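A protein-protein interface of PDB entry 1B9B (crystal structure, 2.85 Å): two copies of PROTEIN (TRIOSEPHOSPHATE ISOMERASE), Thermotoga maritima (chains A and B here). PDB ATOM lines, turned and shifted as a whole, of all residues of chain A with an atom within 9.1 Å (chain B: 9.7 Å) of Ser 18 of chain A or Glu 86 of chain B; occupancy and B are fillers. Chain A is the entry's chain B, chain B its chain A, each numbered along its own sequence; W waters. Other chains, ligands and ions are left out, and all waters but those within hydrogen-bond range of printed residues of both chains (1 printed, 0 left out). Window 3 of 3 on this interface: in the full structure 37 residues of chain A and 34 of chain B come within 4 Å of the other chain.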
ATOM      1  N   TRP A  11     -36.871  -7.577  -3.342  1.00  0.00           N
ATOM      2  CA  TRP A  11     -36.660  -8.184  -4.656  1.00  0.00           C
ATOM      3  C   TRP A  11     -36.100  -9.594  -4.546  1.00  0.00           C
ATOM      4  O   TRP A  11     -36.416 -10.458  -5.364  1.00  0.00           O
ATOM      5  CB  TRP A  11     -35.695  -7.351  -5.509  1.00  0.00           C
ATOM      6  CG  TRP A  11     -36.148  -5.956  -5.839  1.00  0.00           C
ATOM      7  CD1 TRP A  11     -37.216  -5.285  -5.309  1.00  0.00           C
ATOM      8  CD2 TRP A  11     -35.459  -5.015  -6.670  1.00  0.00           C
ATOM      9  NE1 TRP A  11     -37.223  -3.981  -5.746  1.00  0.00           N
ATOM     10  CE2 TRP A  11     -36.155  -3.788  -6.581  1.00  0.00           C
ATOM     11  CE3 TRP A  11     -34.316  -5.088  -7.475  1.00  0.00           C
ATOM     12  CZ2 TRP A  11     -35.740  -2.639  -7.270  1.00  0.00           C
ATOM     13  CZ3 TRP A  11     -33.904  -3.944  -8.161  1.00  0.00           C
ATOM     14  CH2 TRP A  11     -34.616  -2.736  -8.049  1.00  0.00           C
ATOM     15  N   HIS A  14     -33.133 -11.446  -7.709  1.00  0.00           N
ATOM     16  CA  HIS A  14     -33.787 -11.333  -9.010  1.00  0.00           C
ATOM     17  C   HIS A  14     -33.353 -10.374 -10.113  1.00  0.00           C
ATOM     18  O   HIS A  14     -33.456 -10.724 -11.292  1.00  0.00           O
ATOM     19  CB  HIS A  14     -35.294 -11.153  -8.795  1.00  0.00           C
ATOM     20  CG  HIS A  14     -36.001 -12.425  -8.442  1.00  0.00           C
ATOM     21  ND1 HIS A  14     -36.639 -12.616  -7.234  1.00  0.00           N
ATOM     22  CD2 HIS A  14     -36.142 -13.585  -9.127  1.00  0.00           C
ATOM     23  CE1 HIS A  14     -37.141 -13.838  -7.191  1.00  0.00           C
ATOM     24  NE2 HIS A  14     -36.853 -14.447  -8.328  1.00  0.00           N
ATOM     25  N   LYS A  15     -32.870  -9.183  -9.796  1.00  0.00           N
ATOM     26  CA  LYS A  15     -32.527  -8.305 -10.909  1.00  0.00           C
ATOM     27  C   LYS A  15     -31.065  -7.954 -11.159  1.00  0.00           C
ATOM     28  O   LYS A  15     -30.231  -7.998 -10.258  1.00  0.00           O
ATOM     29  CB  LYS A  15     -33.373  -7.029 -10.819  1.00  0.00           C
ATOM     30  CG  LYS A  15     -34.872  -7.334 -10.793  1.00  0.00           C
ATOM     31  CD  LYS A  15     -35.741  -6.118 -11.083  1.00  0.00           C
ATOM     32  CE  LYS A  15     -37.217  -6.499 -11.037  1.00  0.00           C
ATOM     33  NZ  LYS A  15     -37.502  -7.757 -11.805  1.00  0.00           N
ATOM     34  N   THR A  16     -30.774  -7.616 -12.413  1.00  0.00           N
ATOM     35  CA  THR A  16     -29.435  -7.226 -12.849  1.00  0.00           C
ATOM     36  C   THR A  16     -29.398  -5.708 -12.894  1.00  0.00           C
ATOM     37  O   THR A  16     -30.440  -5.070 -13.022  1.00  0.00           O
ATOM     38  CB  THR A  16     -29.137  -7.741 -14.251  1.00  0.00           C
ATOM     39  OG1 THR A  16     -30.146  -7.259 -15.148  1.00  0.00           O
ATOM     40  CG2 THR A  16     -29.126  -9.259 -14.272  1.00  0.00           C
ATOM     41  N   ILE A  17     -28.206  -5.130 -12.806  1.00  0.00           N
ATOM     42  CA  ILE A  17     -28.074  -3.678 -12.814  1.00  0.00           C
ATOM     43  C   ILE A  17     -28.920  -2.990 -13.884  1.00  0.00           C
ATOM     44  O   ILE A  17     -29.403  -1.879 -13.680  1.00  0.00           O
ATOM     45  CB  ILE A  17     -26.611  -3.251 -12.994  1.00  0.00           C
ATOM     46  CG1 ILE A  17     -25.761  -3.830 -11.863  1.00  0.00           C
ATOM     47  CG2 ILE A  17     -26.514  -1.728 -13.005  1.00  0.00           C
ATOM     48  CD1 ILE A  17     -24.352  -3.258 -11.790  1.00  0.00           C
ATOM     49  N   SER A  18     -29.105  -3.649 -15.021  1.00  0.00           N
ATOM     50  CA  SER A  18     -29.904  -3.074 -16.096  1.00  0.00           C
ATOM     51  C   SER A  18     -31.384  -3.075 -15.712  1.00  0.00           C
ATOM     52  O   SER A  18     -31.982  -2.015 -15.526  1.00  0.00           O
ATOM     53  CB  SER A  18     -29.696  -3.865 -17.388  1.00  0.00           C
ATOM     54  OG  SER A  18     -30.051  -5.226 -17.209  1.00  0.00           O
ATOM     55  N   GLU A  19     -31.967  -4.267 -15.590  1.00  0.00           N
ATOM     56  CA  GLU A  19     -33.372  -4.397 -15.218  1.00  0.00           C
ATOM     57  C   GLU A  19     -33.675  -3.497 -14.026  1.00  0.00           C
ATOM     58  O   GLU A  19     -34.741  -2.892 -13.934  1.00  0.00           O
ATOM     59  CB  GLU A  19     -33.678  -5.846 -14.856  1.00  0.00           C
ATOM     60  CG  GLU A  19     -33.328  -6.824 -15.948  1.00  0.00           C
ATOM     61  CD  GLU A  19     -33.473  -8.265 -15.509  1.00  0.00           C
ATOM     62  OE1 GLU A  19     -32.731  -8.687 -14.600  1.00  0.00           O
ATOM     63  OE2 GLU A  19     -34.330  -8.980 -16.071  1.00  0.00           O
ATOM     64  N   ALA A  20     -32.714  -3.410 -13.115  1.00  0.00           N
ATOM     65  CA  ALA A  20     -32.855  -2.595 -11.926  1.00  0.00           C
ATOM     66  C   ALA A  20     -32.966  -1.107 -12.256  1.00  0.00           C
ATOM     67  O   ALA A  20     -33.949  -0.463 -11.887  1.00  0.00           O
ATOM     68  CB  ALA A  20     -31.682  -2.838 -10.994  1.00  0.00           C
ATOM     69  N   LYS A  21     -31.964  -0.562 -12.944  1.00  0.00           N
ATOM     70  CA  LYS A  21     -31.958   0.861 -13.302  1.00  0.00           C
ATOM     71  C   LYS A  21     -33.257   1.289 -13.974  1.00  0.00           C
ATOM     72  O   LYS A  21     -33.760   2.391 -13.739  1.00  0.00           O
ATOM     73  CB  LYS A  21     -30.781   1.184 -14.235  1.00  0.00           C
ATOM     74  CG  LYS A  21     -29.408   1.075 -13.590  1.00  0.00           C
ATOM     75  CD  LYS A  21     -28.289   1.437 -14.566  1.00  0.00           C
ATOM     76  CE  LYS A  21     -28.118   2.940 -14.698  1.00  0.00           C
ATOM     77  NZ  LYS A  21     -27.701   3.572 -13.412  1.00  0.00           N
ATOM     78  N   LYS A  22     -33.790   0.408 -14.815  1.00  0.00           N
ATOM     79  CA  LYS A  22     -35.027   0.673 -15.531  1.00  0.00           C
ATOM     80  C   LYS A  22     -36.166   0.829 -14.539  1.00  0.00           C
ATOM     81  O   LYS A  22     -36.651   1.936 -14.293  1.00  0.00           O
ATOM     82  CB  LYS A  22     -35.324  -0.482 -16.493  1.00  0.00           C
ATOM     83  CG  LYS A  22     -34.199  -0.726 -17.482  1.00  0.00           C
ATOM     84  CD  LYS A  22     -34.515  -1.827 -18.478  1.00  0.00           C
ATOM     85  CE  LYS A  22     -33.379  -1.962 -19.493  1.00  0.00           C
ATOM     86  NZ  LYS A  22     -33.684  -2.930 -20.588  1.00  0.00           N
ATOM     87  N   PHE A  23     -36.572  -0.299 -13.967  1.00  0.00           N
ATOM     88  CA  PHE A  23     -37.651  -0.359 -12.993  1.00  0.00           C
ATOM     89  C   PHE A  23     -37.636   0.801 -11.992  1.00  0.00           C
ATOM     90  O   PHE A  23     -38.668   1.410 -11.720  1.00  0.00           O
ATOM     91  CB  PHE A  23     -37.568  -1.686 -12.247  1.00  0.00           C
ATOM     92  CG  PHE A  23     -38.743  -1.961 -11.371  1.00  0.00           C
ATOM     93  CD1 PHE A  23     -39.916  -1.225 -11.495  1.00  0.00           C
ATOM     94  CD2 PHE A  23     -38.678  -2.955 -10.403  1.00  0.00           C
ATOM     95  CE1 PHE A  23     -41.008  -1.475 -10.663  1.00  0.00           C
ATOM     96  CE2 PHE A  23     -39.764  -3.211  -9.567  1.00  0.00           C
ATOM     97  CZ  PHE A  23     -40.931  -2.468  -9.699  1.00  0.00           C
ATOM     98  N   VAL A  24     -36.464   1.106 -11.452  1.00  0.00           N
ATOM     99  CA  VAL A  24     -36.332   2.177 -10.473  1.00  0.00           C
ATOM    100  C   VAL A  24     -36.737   3.557 -11.008  1.00  0.00           C
ATOM    101  O   VAL A  24     -37.526   4.270 -10.380  1.00  0.00           O
ATOM    102  CB  VAL A  24     -34.886   2.222  -9.922  1.00  0.00           C
ATOM    103  CG1 VAL A  24     -34.721   3.389  -8.972  1.00  0.00           C
ATOM    104  CG2 VAL A  24     -34.570   0.913  -9.200  1.00  0.00           C
ATOM    105  N   SER A  25     -36.200   3.936 -12.165  1.00  0.00           N
ATOM    106  CA  SER A  25     -36.538   5.224 -12.769  1.00  0.00           C
ATOM    107  C   SER A  25     -38.051   5.298 -12.966  1.00  0.00           C
ATOM    108  O   SER A  25     -38.687   6.296 -12.618  1.00  0.00           O
ATOM    109  CB  SER A  25     -35.833   5.382 -14.116  1.00  0.00           C
ATOM    110  OG  SER A  25     -34.430   5.308 -13.956  1.00  0.00           O
ATOM    111  N   THR A  46     -25.083  -6.344  -5.560  1.00  0.00           N
ATOM    112  CA  THR A  46     -24.492  -6.041  -6.855  1.00  0.00           C
ATOM    113  C   THR A  46     -25.058  -4.771  -7.468  1.00  0.00           C
ATOM    114  O   THR A  46     -24.311  -3.951  -8.003  1.00  0.00           O
ATOM    115  CB  THR A  46     -24.710  -7.198  -7.850  1.00  0.00           C
ATOM    116  OG1 THR A  46     -26.116  -7.412  -8.043  1.00  0.00           O
ATOM    117  CG2 THR A  46     -24.061  -8.473  -7.334  1.00  0.00           C
ATOM    118  N   ALA A  47     -26.374  -4.600  -7.363  1.00  0.00           N
ATOM    119  CA  ALA A  47     -27.052  -3.444  -7.944  1.00  0.00           C
ATOM    120  C   ALA A  47     -27.537  -2.346  -6.998  1.00  0.00           C
ATOM    121  O   ALA A  47     -28.594  -1.772  -7.227  1.00  0.00           O
ATOM    122  CB  ALA A  47     -28.219  -3.928  -8.778  1.00  0.00           C
ATOM    123  N   GLU A  50     -25.923   1.555  -8.312  1.00  0.00           N
ATOM    124  CA  GLU A  50     -26.599   2.070  -9.488  1.00  0.00           C
ATOM    125  C   GLU A  50     -27.945   2.664  -9.085  1.00  0.00           C
ATOM    126  O   GLU A  50     -28.195   3.858  -9.292  1.00  0.00           O
ATOM    127  CB  GLU A  50     -26.778   0.944 -10.507  1.00  0.00           C
ATOM    128  CG  GLU A  50     -26.385   1.329 -11.927  1.00  0.00           C
ATOM    129  CD  GLU A  50     -24.987   1.919 -12.019  1.00  0.00           C
ATOM    130  OE1 GLU A  50     -24.023   1.244 -11.596  1.00  0.00           O
ATOM    131  OE2 GLU A  50     -24.852   3.058 -12.516  1.00  0.00           O
ATOM    132  N   VAL A  51     -28.802   1.827  -8.502  1.00  0.00           N
ATOM    133  CA  VAL A  51     -30.115   2.256  -8.037  1.00  0.00           C
ATOM    134  C   VAL A  51     -29.914   3.413  -7.069  1.00  0.00           C
ATOM    135  O   VAL A  51     -30.725   4.329  -6.985  1.00  0.00           O
ATOM    136  CB  VAL A  51     -30.841   1.110  -7.301  1.00  0.00           C
ATOM    137  CG1 VAL A  51     -32.045   1.650  -6.556  1.00  0.00           C
ATOM    138  CG2 VAL A  51     -31.273   0.038  -8.295  1.00  0.00           C
ATOM    139  N   ILE A  54     -30.074   6.694  -8.760  1.00  0.00           N
ATOM    140  CA  ILE A  54     -31.388   6.943  -9.345  1.00  0.00           C
ATOM    141  C   ILE A  54     -32.362   7.405  -8.253  1.00  0.00           C
ATOM    142  O   ILE A  54     -33.491   7.804  -8.540  1.00  0.00           O
ATOM    143  CB  ILE A  54     -31.966   5.669 -10.002  1.00  0.00           C
ATOM    144  CG1 ILE A  54     -31.050   5.207 -11.129  1.00  0.00           C
ATOM    145  CG2 ILE A  54     -33.363   5.940 -10.549  1.00  0.00           C
ATOM    146  CD1 ILE A  54     -31.552   3.965 -11.844  1.00  0.00           C
ATOM    147  N   LEU B  48     -18.581  -4.021  -6.900  1.00  0.00           N
ATOM    148  CA  LEU B  48     -18.275  -4.734  -8.131  1.00  0.00           C
ATOM    149  C   LEU B  48     -18.457  -3.948  -9.422  1.00  0.00           C
ATOM    150  O   LEU B  48     -17.514  -3.816 -10.194  1.00  0.00           O
ATOM    151  CB  LEU B  48     -19.068  -6.036  -8.223  1.00  0.00           C
ATOM    152  CG  LEU B  48     -18.606  -7.148  -7.284  1.00  0.00           C
ATOM    153  CD1 LEU B  48     -19.284  -8.455  -7.681  1.00  0.00           C
ATOM    154  CD2 LEU B  48     -17.086  -7.280  -7.349  1.00  0.00           C
ATOM    155  N   SER B  49     -19.649  -3.421  -9.671  1.00  0.00           N
ATOM    156  CA  SER B  49     -19.856  -2.693 -10.913  1.00  0.00           C
ATOM    157  C   SER B  49     -18.949  -1.471 -11.063  1.00  0.00           C
ATOM    158  O   SER B  49     -18.421  -1.220 -12.141  1.00  0.00           O
ATOM    159  CB  SER B  49     -21.317  -2.275 -11.055  1.00  0.00           C
ATOM    160  OG  SER B  49     -21.660  -1.329 -10.072  1.00  0.00           O
ATOM    161  N   GLY B  52     -15.767  -2.691 -11.983  1.00  0.00           N
ATOM    162  CA  GLY B  52     -15.849  -3.289 -13.299  1.00  0.00           C
ATOM    163  C   GLY B  52     -15.415  -2.305 -14.365  1.00  0.00           C
ATOM    164  O   GLY B  52     -14.651  -2.660 -15.254  1.00  0.00           O
ATOM    165  N   GLU B  53     -15.895  -1.069 -14.269  1.00  0.00           N
ATOM    166  CA  GLU B  53     -15.549  -0.026 -15.230  1.00  0.00           C
ATOM    167  C   GLU B  53     -14.043   0.182 -15.278  1.00  0.00           C
ATOM    168  O   GLU B  53     -13.402  -0.072 -16.293  1.00  0.00           O
ATOM    169  CB  GLU B  53     -16.181   1.309 -14.846  1.00  0.00           C
ATOM    170  CG  GLU B  53     -17.635   1.262 -14.430  1.00  0.00           C
ATOM    171  CD  GLU B  53     -18.547   0.629 -15.481  1.00  0.00           C
ATOM    172  OE1 GLU B  53     -18.543   1.083 -16.670  1.00  0.00           O
ATOM    173  OE2 GLU B  53     -19.280  -0.325 -15.094  1.00  0.00           O
ATOM    174  N   SER B  56     -12.628  -2.705 -17.033  1.00  0.00           N
ATOM    175  CA  SER B  56     -13.074  -3.044 -18.385  1.00  0.00           C
ATOM    176  C   SER B  56     -12.019  -2.701 -19.420  1.00  0.00           C
ATOM    177  O   SER B  56     -11.583  -1.551 -19.521  1.00  0.00           O
ATOM    178  CB  SER B  56     -14.369  -2.310 -18.728  1.00  0.00           C
ATOM    179  OG  SER B  56     -15.416  -2.697 -17.857  1.00  0.00           O
ATOM    180  N   LEU B  62     -11.586  -8.965 -12.825  1.00  0.00           N
ATOM    181  CA  LEU B  62     -12.531  -8.881 -11.715  1.00  0.00           C
ATOM    182  C   LEU B  62     -12.902 -10.200 -11.064  1.00  0.00           C
ATOM    183  O   LEU B  62     -13.270 -11.157 -11.745  1.00  0.00           O
ATOM    184  CB  LEU B  62     -13.820  -8.210 -12.183  1.00  0.00           C
ATOM    185  CG  LEU B  62     -14.461  -7.172 -11.261  1.00  0.00           C
ATOM    186  CD1 LEU B  62     -15.938  -7.078 -11.612  1.00  0.00           C
ATOM    187  CD2 LEU B  62     -14.292  -7.562  -9.802  1.00  0.00           C
ATOM    188  N   ILE B  79     -26.437 -13.511  -3.951  1.00  0.00           N
ATOM    189  CA  ILE B  79     -26.139 -13.006  -5.292  1.00  0.00           C
ATOM    190  C   ILE B  79     -26.037 -14.179  -6.263  1.00  0.00           C
ATOM    191  O   ILE B  79     -25.396 -15.182  -5.964  1.00  0.00           O
ATOM    192  CB  ILE B  79     -24.813 -12.237  -5.334  1.00  0.00           C
ATOM    193  CG1 ILE B  79     -24.849 -11.074  -4.345  1.00  0.00           C
ATOM    194  CG2 ILE B  79     -24.570 -11.719  -6.735  1.00  0.00           C
ATOM    195  CD1 ILE B  79     -25.956 -10.070  -4.591  1.00  0.00           C
ATOM    196  N   SER B  80     -26.667 -14.047  -7.426  1.00  0.00           N
ATOM    197  CA  SER B  80     -26.660 -15.111  -8.433  1.00  0.00           C
ATOM    198  C   SER B  80     -25.477 -15.025  -9.386  1.00  0.00           C
ATOM    199  O   SER B  80     -24.805 -13.993  -9.474  1.00  0.00           O
ATOM    200  CB  SER B  80     -27.947 -15.068  -9.267  1.00  0.00           C
ATOM    201  OG  SER B  80     -27.985 -13.911 -10.095  1.00  0.00           O
ATOM    202  N   PRO B  81     -25.206 -16.120 -10.115  1.00  0.00           N
ATOM    203  CA  PRO B  81     -24.099 -16.157 -11.073  1.00  0.00           C
ATOM    204  C   PRO B  81     -24.344 -15.107 -12.155  1.00  0.00           C
ATOM    205  O   PRO B  81     -23.416 -14.428 -12.603  1.00  0.00           O
ATOM    206  CB  PRO B  81     -24.173 -17.574 -11.619  1.00  0.00           C
ATOM    207  CG  PRO B  81     -24.689 -18.344 -10.452  1.00  0.00           C
ATOM    208  CD  PRO B  81     -25.798 -17.457  -9.958  1.00  0.00           C
ATOM    209  N   LEU B  82     -25.607 -14.979 -12.557  1.00  0.00           N
ATOM    210  CA  LEU B  82     -25.997 -14.008 -13.570  1.00  0.00           C
ATOM    211  C   LEU B  82     -25.534 -12.615 -13.203  1.00  0.00           C
ATOM    212  O   LEU B  82     -24.916 -11.927 -14.005  1.00  0.00           O
ATOM    213  CB  LEU B  82     -27.513 -13.969 -13.737  1.00  0.00           C
ATOM    214  CG  LEU B  82     -28.214 -15.099 -14.476  1.00  0.00           C
ATOM    215  CD1 LEU B  82     -29.662 -14.691 -14.711  1.00  0.00           C
ATOM    216  CD2 LEU B  82     -27.519 -15.363 -15.803  1.00  0.00           C
ATOM    217  N   MET B  83     -25.854 -12.199 -11.984  1.00  0.00           N
ATOM    218  CA  MET B  83     -25.490 -10.875 -11.514  1.00  0.00           C
ATOM    219  C   MET B  83     -23.989 -10.616 -11.565  1.00  0.00           C
ATOM    220  O   MET B  83     -23.561  -9.486 -11.817  1.00  0.00           O
ATOM    221  CB  MET B  83     -26.014 -10.673 -10.095  1.00  0.00           C
ATOM    222  CG  MET B  83     -27.525 -10.528 -10.022  1.00  0.00           C
ATOM    223  SD  MET B  83     -28.165 -10.613  -8.338  1.00  0.00           S
ATOM    224  CE  MET B  83     -29.401 -11.873  -8.518  1.00  0.00           C
ATOM    225  N   LEU B  84     -23.198 -11.662 -11.332  1.00  0.00           N
ATOM    226  CA  LEU B  84     -21.742 -11.538 -11.358  1.00  0.00           C
ATOM    227  C   LEU B  84     -21.248 -11.441 -12.801  1.00  0.00           C
ATOM    228  O   LEU B  84     -20.386 -10.618 -13.126  1.00  0.00           O
ATOM    229  CB  LEU B  84     -21.086 -12.742 -10.676  1.00  0.00           C
ATOM    230  CG  LEU B  84     -21.407 -13.009  -9.204  1.00  0.00           C
ATOM    231  CD1 LEU B  84     -20.774 -14.330  -8.795  1.00  0.00           C
ATOM    232  CD2 LEU B  84     -20.902 -11.871  -8.325  1.00  0.00           C
ATOM    233  N   GLN B  85     -21.806 -12.291 -13.657  1.00  0.00           N
ATOM    234  CA  GLN B  85     -21.450 -12.328 -15.073  1.00  0.00           C
ATOM    235  C   GLN B  85     -21.682 -10.978 -15.737  1.00  0.00           C
ATOM    236  O   GLN B  85     -20.761 -10.386 -16.295  1.00  0.00           O
ATOM    237  CB  GLN B  85     -22.276 -13.401 -15.775  1.00  0.00           C
ATOM    238  CG  GLN B  85     -21.986 -13.561 -17.243  1.00  0.00           C
ATOM    239  CD  GLN B  85     -22.665 -14.788 -17.811  1.00  0.00           C
ATOM    240  OE1 GLN B  85     -23.886 -14.928 -17.726  1.00  0.00           O
ATOM    241  NE2 GLN B  85     -21.879 -15.689 -18.389  1.00  0.00           N
ATOM    242  N   GLU B  86     -22.919 -10.496 -15.670  1.00  0.00           N
ATOM    243  CA  GLU B  86     -23.277  -9.209 -16.253  1.00  0.00           C
ATOM    244  C   GLU B  86     -22.287  -8.105 -15.875  1.00  0.00           C
ATOM    245  O   GLU B  86     -22.168  -7.110 -16.578  1.00  0.00           O
ATOM    246  CB  GLU B  86     -24.685  -8.790 -15.813  1.00  0.00           C
ATOM    247  CG  GLU B  86     -25.034  -7.356 -16.203  1.00  0.00           C
ATOM    248  CD  GLU B  86     -26.087  -6.721 -15.313  1.00  0.00           C
ATOM    249  OE1 GLU B  86     -25.923  -6.730 -14.074  1.00  0.00           O
ATOM    250  OE2 GLU B  86     -27.077  -6.198 -15.855  1.00  0.00           O
ATOM    251  N   ILE B  87     -21.581  -8.266 -14.764  1.00  0.00           N
ATOM    252  CA  ILE B  87     -20.625  -7.240 -14.361  1.00  0.00           C
ATOM    253  C   ILE B  87     -19.236  -7.555 -14.919  1.00  0.00           C
ATOM    254  O   ILE B  87     -18.322  -6.735 -14.842  1.00  0.00           O
ATOM    255  CB  ILE B  87     -20.554  -7.101 -12.817  1.00  0.00           C
ATOM    256  CG1 ILE B  87     -21.945  -6.811 -12.261  1.00  0.00           C
ATOM    257  CG2 ILE B  87     -19.635  -5.956 -12.428  1.00  0.00           C
ATOM    258  CD1 ILE B  87     -21.962  -6.530 -10.778  1.00  0.00           C
ATOM    259  N   GLY B  88     -19.084  -8.745 -15.490  1.00  0.00           N
ATOM    260  CA  GLY B  88     -17.804  -9.119 -16.057  1.00  0.00           C
ATOM    261  C   GLY B  88     -16.840  -9.731 -15.065  1.00  0.00           C
ATOM    262  O   GLY B  88     -15.628  -9.562 -15.173  1.00  0.00           O
ATOM    263  N   VAL B  89     -17.376 -10.438 -14.083  1.00  0.00           N
ATOM    264  CA  VAL B  89     -16.541 -11.083 -13.086  1.00  0.00           C
ATOM    265  C   VAL B  89     -16.069 -12.385 -13.717  1.00  0.00           C
ATOM    266  O   VAL B  89     -16.880 -13.162 -14.212  1.00  0.00           O
ATOM    267  CB  VAL B  89     -17.350 -11.385 -11.801  1.00  0.00           C
ATOM    268  CG1 VAL B  89     -16.489 -12.132 -10.804  1.00  0.00           C
ATOM    269  CG2 VAL B  89     -17.850 -10.085 -11.188  1.00  0.00           C
ATOM    270  N   GLU B  90     -14.761 -12.617 -13.716  1.00  0.00           N
ATOM    271  CA  GLU B  90     -14.216 -13.838 -14.303  1.00  0.00           C
ATOM    272  C   GLU B  90     -13.978 -14.929 -13.265  1.00  0.00           C
ATOM    273  O   GLU B  90     -14.213 -16.106 -13.536  1.00  0.00           O
ATOM    274  CB  GLU B  90     -12.913 -13.546 -15.053  1.00  0.00           C
ATOM    275  CG  GLU B  90     -13.064 -12.584 -16.228  1.00  0.00           C
ATOM    276  CD  GLU B  90     -11.883 -12.638 -17.190  1.00  0.00           C
ATOM    277  OE1 GLU B  90     -11.146 -13.652 -17.188  1.00  0.00           O
ATOM    278  OE2 GLU B  90     -11.700 -11.668 -17.958  1.00  0.00           O
ATOM    279  N   LYS B 120     -21.815 -20.564 -16.192  1.00  0.00           N
ATOM    280  CA  LYS B 120     -21.732 -19.249 -16.809  1.00  0.00           C
ATOM    281  C   LYS B 120     -20.309 -18.944 -17.258  1.00  0.00           C
ATOM    282  O   LYS B 120     -19.900 -17.785 -17.361  1.00  0.00           O
ATOM    283  CB  LYS B 120     -22.246 -18.177 -15.850  1.00  0.00           C
ATOM    284  CG  LYS B 120     -23.764 -18.110 -15.790  1.00  0.00           C
ATOM    285  CD  LYS B 120     -24.378 -19.478 -15.496  1.00  0.00           C
ATOM    286  CE  LYS B 120     -25.886 -19.395 -15.477  1.00  0.00           C
ATOM    287  NZ  LYS B 120     -26.317 -18.268 -14.605  1.00  0.00           N
ATOM    288  N   MET B 122     -17.328 -19.121 -15.883  1.00  0.00           N
ATOM    289  CA  MET B 122     -16.426 -18.362 -15.028  1.00  0.00           C
ATOM    290  C   MET B 122     -15.496 -19.358 -14.366  1.00  0.00           C
ATOM    291  O   MET B 122     -15.759 -20.563 -14.392  1.00  0.00           O
ATOM    292  CB  MET B 122     -17.210 -17.590 -13.972  1.00  0.00           C
ATOM    293  CG  MET B 122     -18.112 -16.526 -14.549  1.00  0.00           C
ATOM    294  SD  MET B 122     -18.902 -15.550 -13.270  1.00  0.00           S
ATOM    295  CE  MET B 122     -20.379 -16.509 -12.995  1.00  0.00           C
HETATM  296  O   HOH W   1     -24.411  -0.933  -8.526  1.00  0.00           O
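Ser 18 of chain A touches just one residue of chain B: Glu 86.
Of chain A, only Thr 16, Ile 17 and Ser 18 come within 4 Å of Glu 86 of chain B.
Printed residues of chain B within 4 Å of Ile 17 of chain A: Ser 49 (3.3 Å) and Glu 86 (3.1 Å).
Of the printed residues of chain B, Glu 50 of chain A touches Ser 49 (3.8 Å).
Printed residues of chain A within 4 Å of Ser 49 of chain B: Ile 17 and Glu 50.
Of the printed residues of chain B, Lys 15 of chain A touches Met 83.
Printed residues of chain B within 4 Å of His 14 of chain A: Met 83.
Printed residues of chain B within 4 Å of Thr 46 of chain A: Ile 79 and Met 83.
The nearest residue of chain B that does not touch Ser 18 of chain A is Ile 87 of chain B (8.3 Å).
Of the 20 printed residues of chain B, 4 touch a printed residue of chain A.
Of the 18 printed residues of chain A, 7 touch a printed residue of chain B.
Hydrophobic or aromatic side chains of chain A within 4 Å of the printed part of chain B: Ile 17.
Among the printed residues, 9 pairs touch across the chains.
Among the printed residues, no Asp or Glu carboxylate lies within 4 Å of a Lys or Arg side-chain nitrogen of the other chain.
The side-chain hydroxyl (OG) of Ser 80 of chain B sits close to the backbone NH (N) of Met 83 of chain B (3.3 Å).
A ring nitrogen (ND1) of His 14 of chain A lies within hydrogen-bond range of the backbone carbonyl oxygen (O) of Trp 11 of chain A (2.9 Å).
OG1 of Thr 16 of chain A sits at hydrogen-bond distance from OG of Ser 18 of chain A (2.9 Å).
The side-chain hydroxyl of Thr 16 of chain A lies within hydrogen-bond range of the side-chain carboxylate of Glu 19 of chain A (3.0 Å).
The side-chain carboxylate of Glu 50 of chain A lies within salt-bridge range of the side-chain amino group of Lys 21 of chain A.
Among the printed residues, merely in contact across the chains: Ile 17 of chain A with Ser 49 of chain B, Thr 46 of chain A with Ile 79 of chain B, Lys 15 of chain A with Met 83 of chain B, Glu 50 of chain A with Ser 49 of chain B, Thr 46 of chain A with Met 83 of chain B and His 14 of chain A with Met 83 of chain B.
OG1 of Thr 16 of chain A sits close to OE2 of Glu 86 of chain B (3.3 Å).
The side-chain carboxylate (OE1) of Glu 86 of chain B is in hydrogen-bond range of the backbone NH (N) of Ile 17 of chain A, at 3.1 Å.
The backbone NH (N) of Ser 18 of chain A is in hydrogen-bond range of the side-chain carboxylate (OE2) of Glu 86 of chain B (3.4 Å).
Water W1 lies within hydrogen-bond range of N of Glu 50 of chain A (2.9 Å), O of Thr 46 of chain A (3.1 Å) and OG of Ser 49 of chain B (3.2 Å).
No position is printed for both chains.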
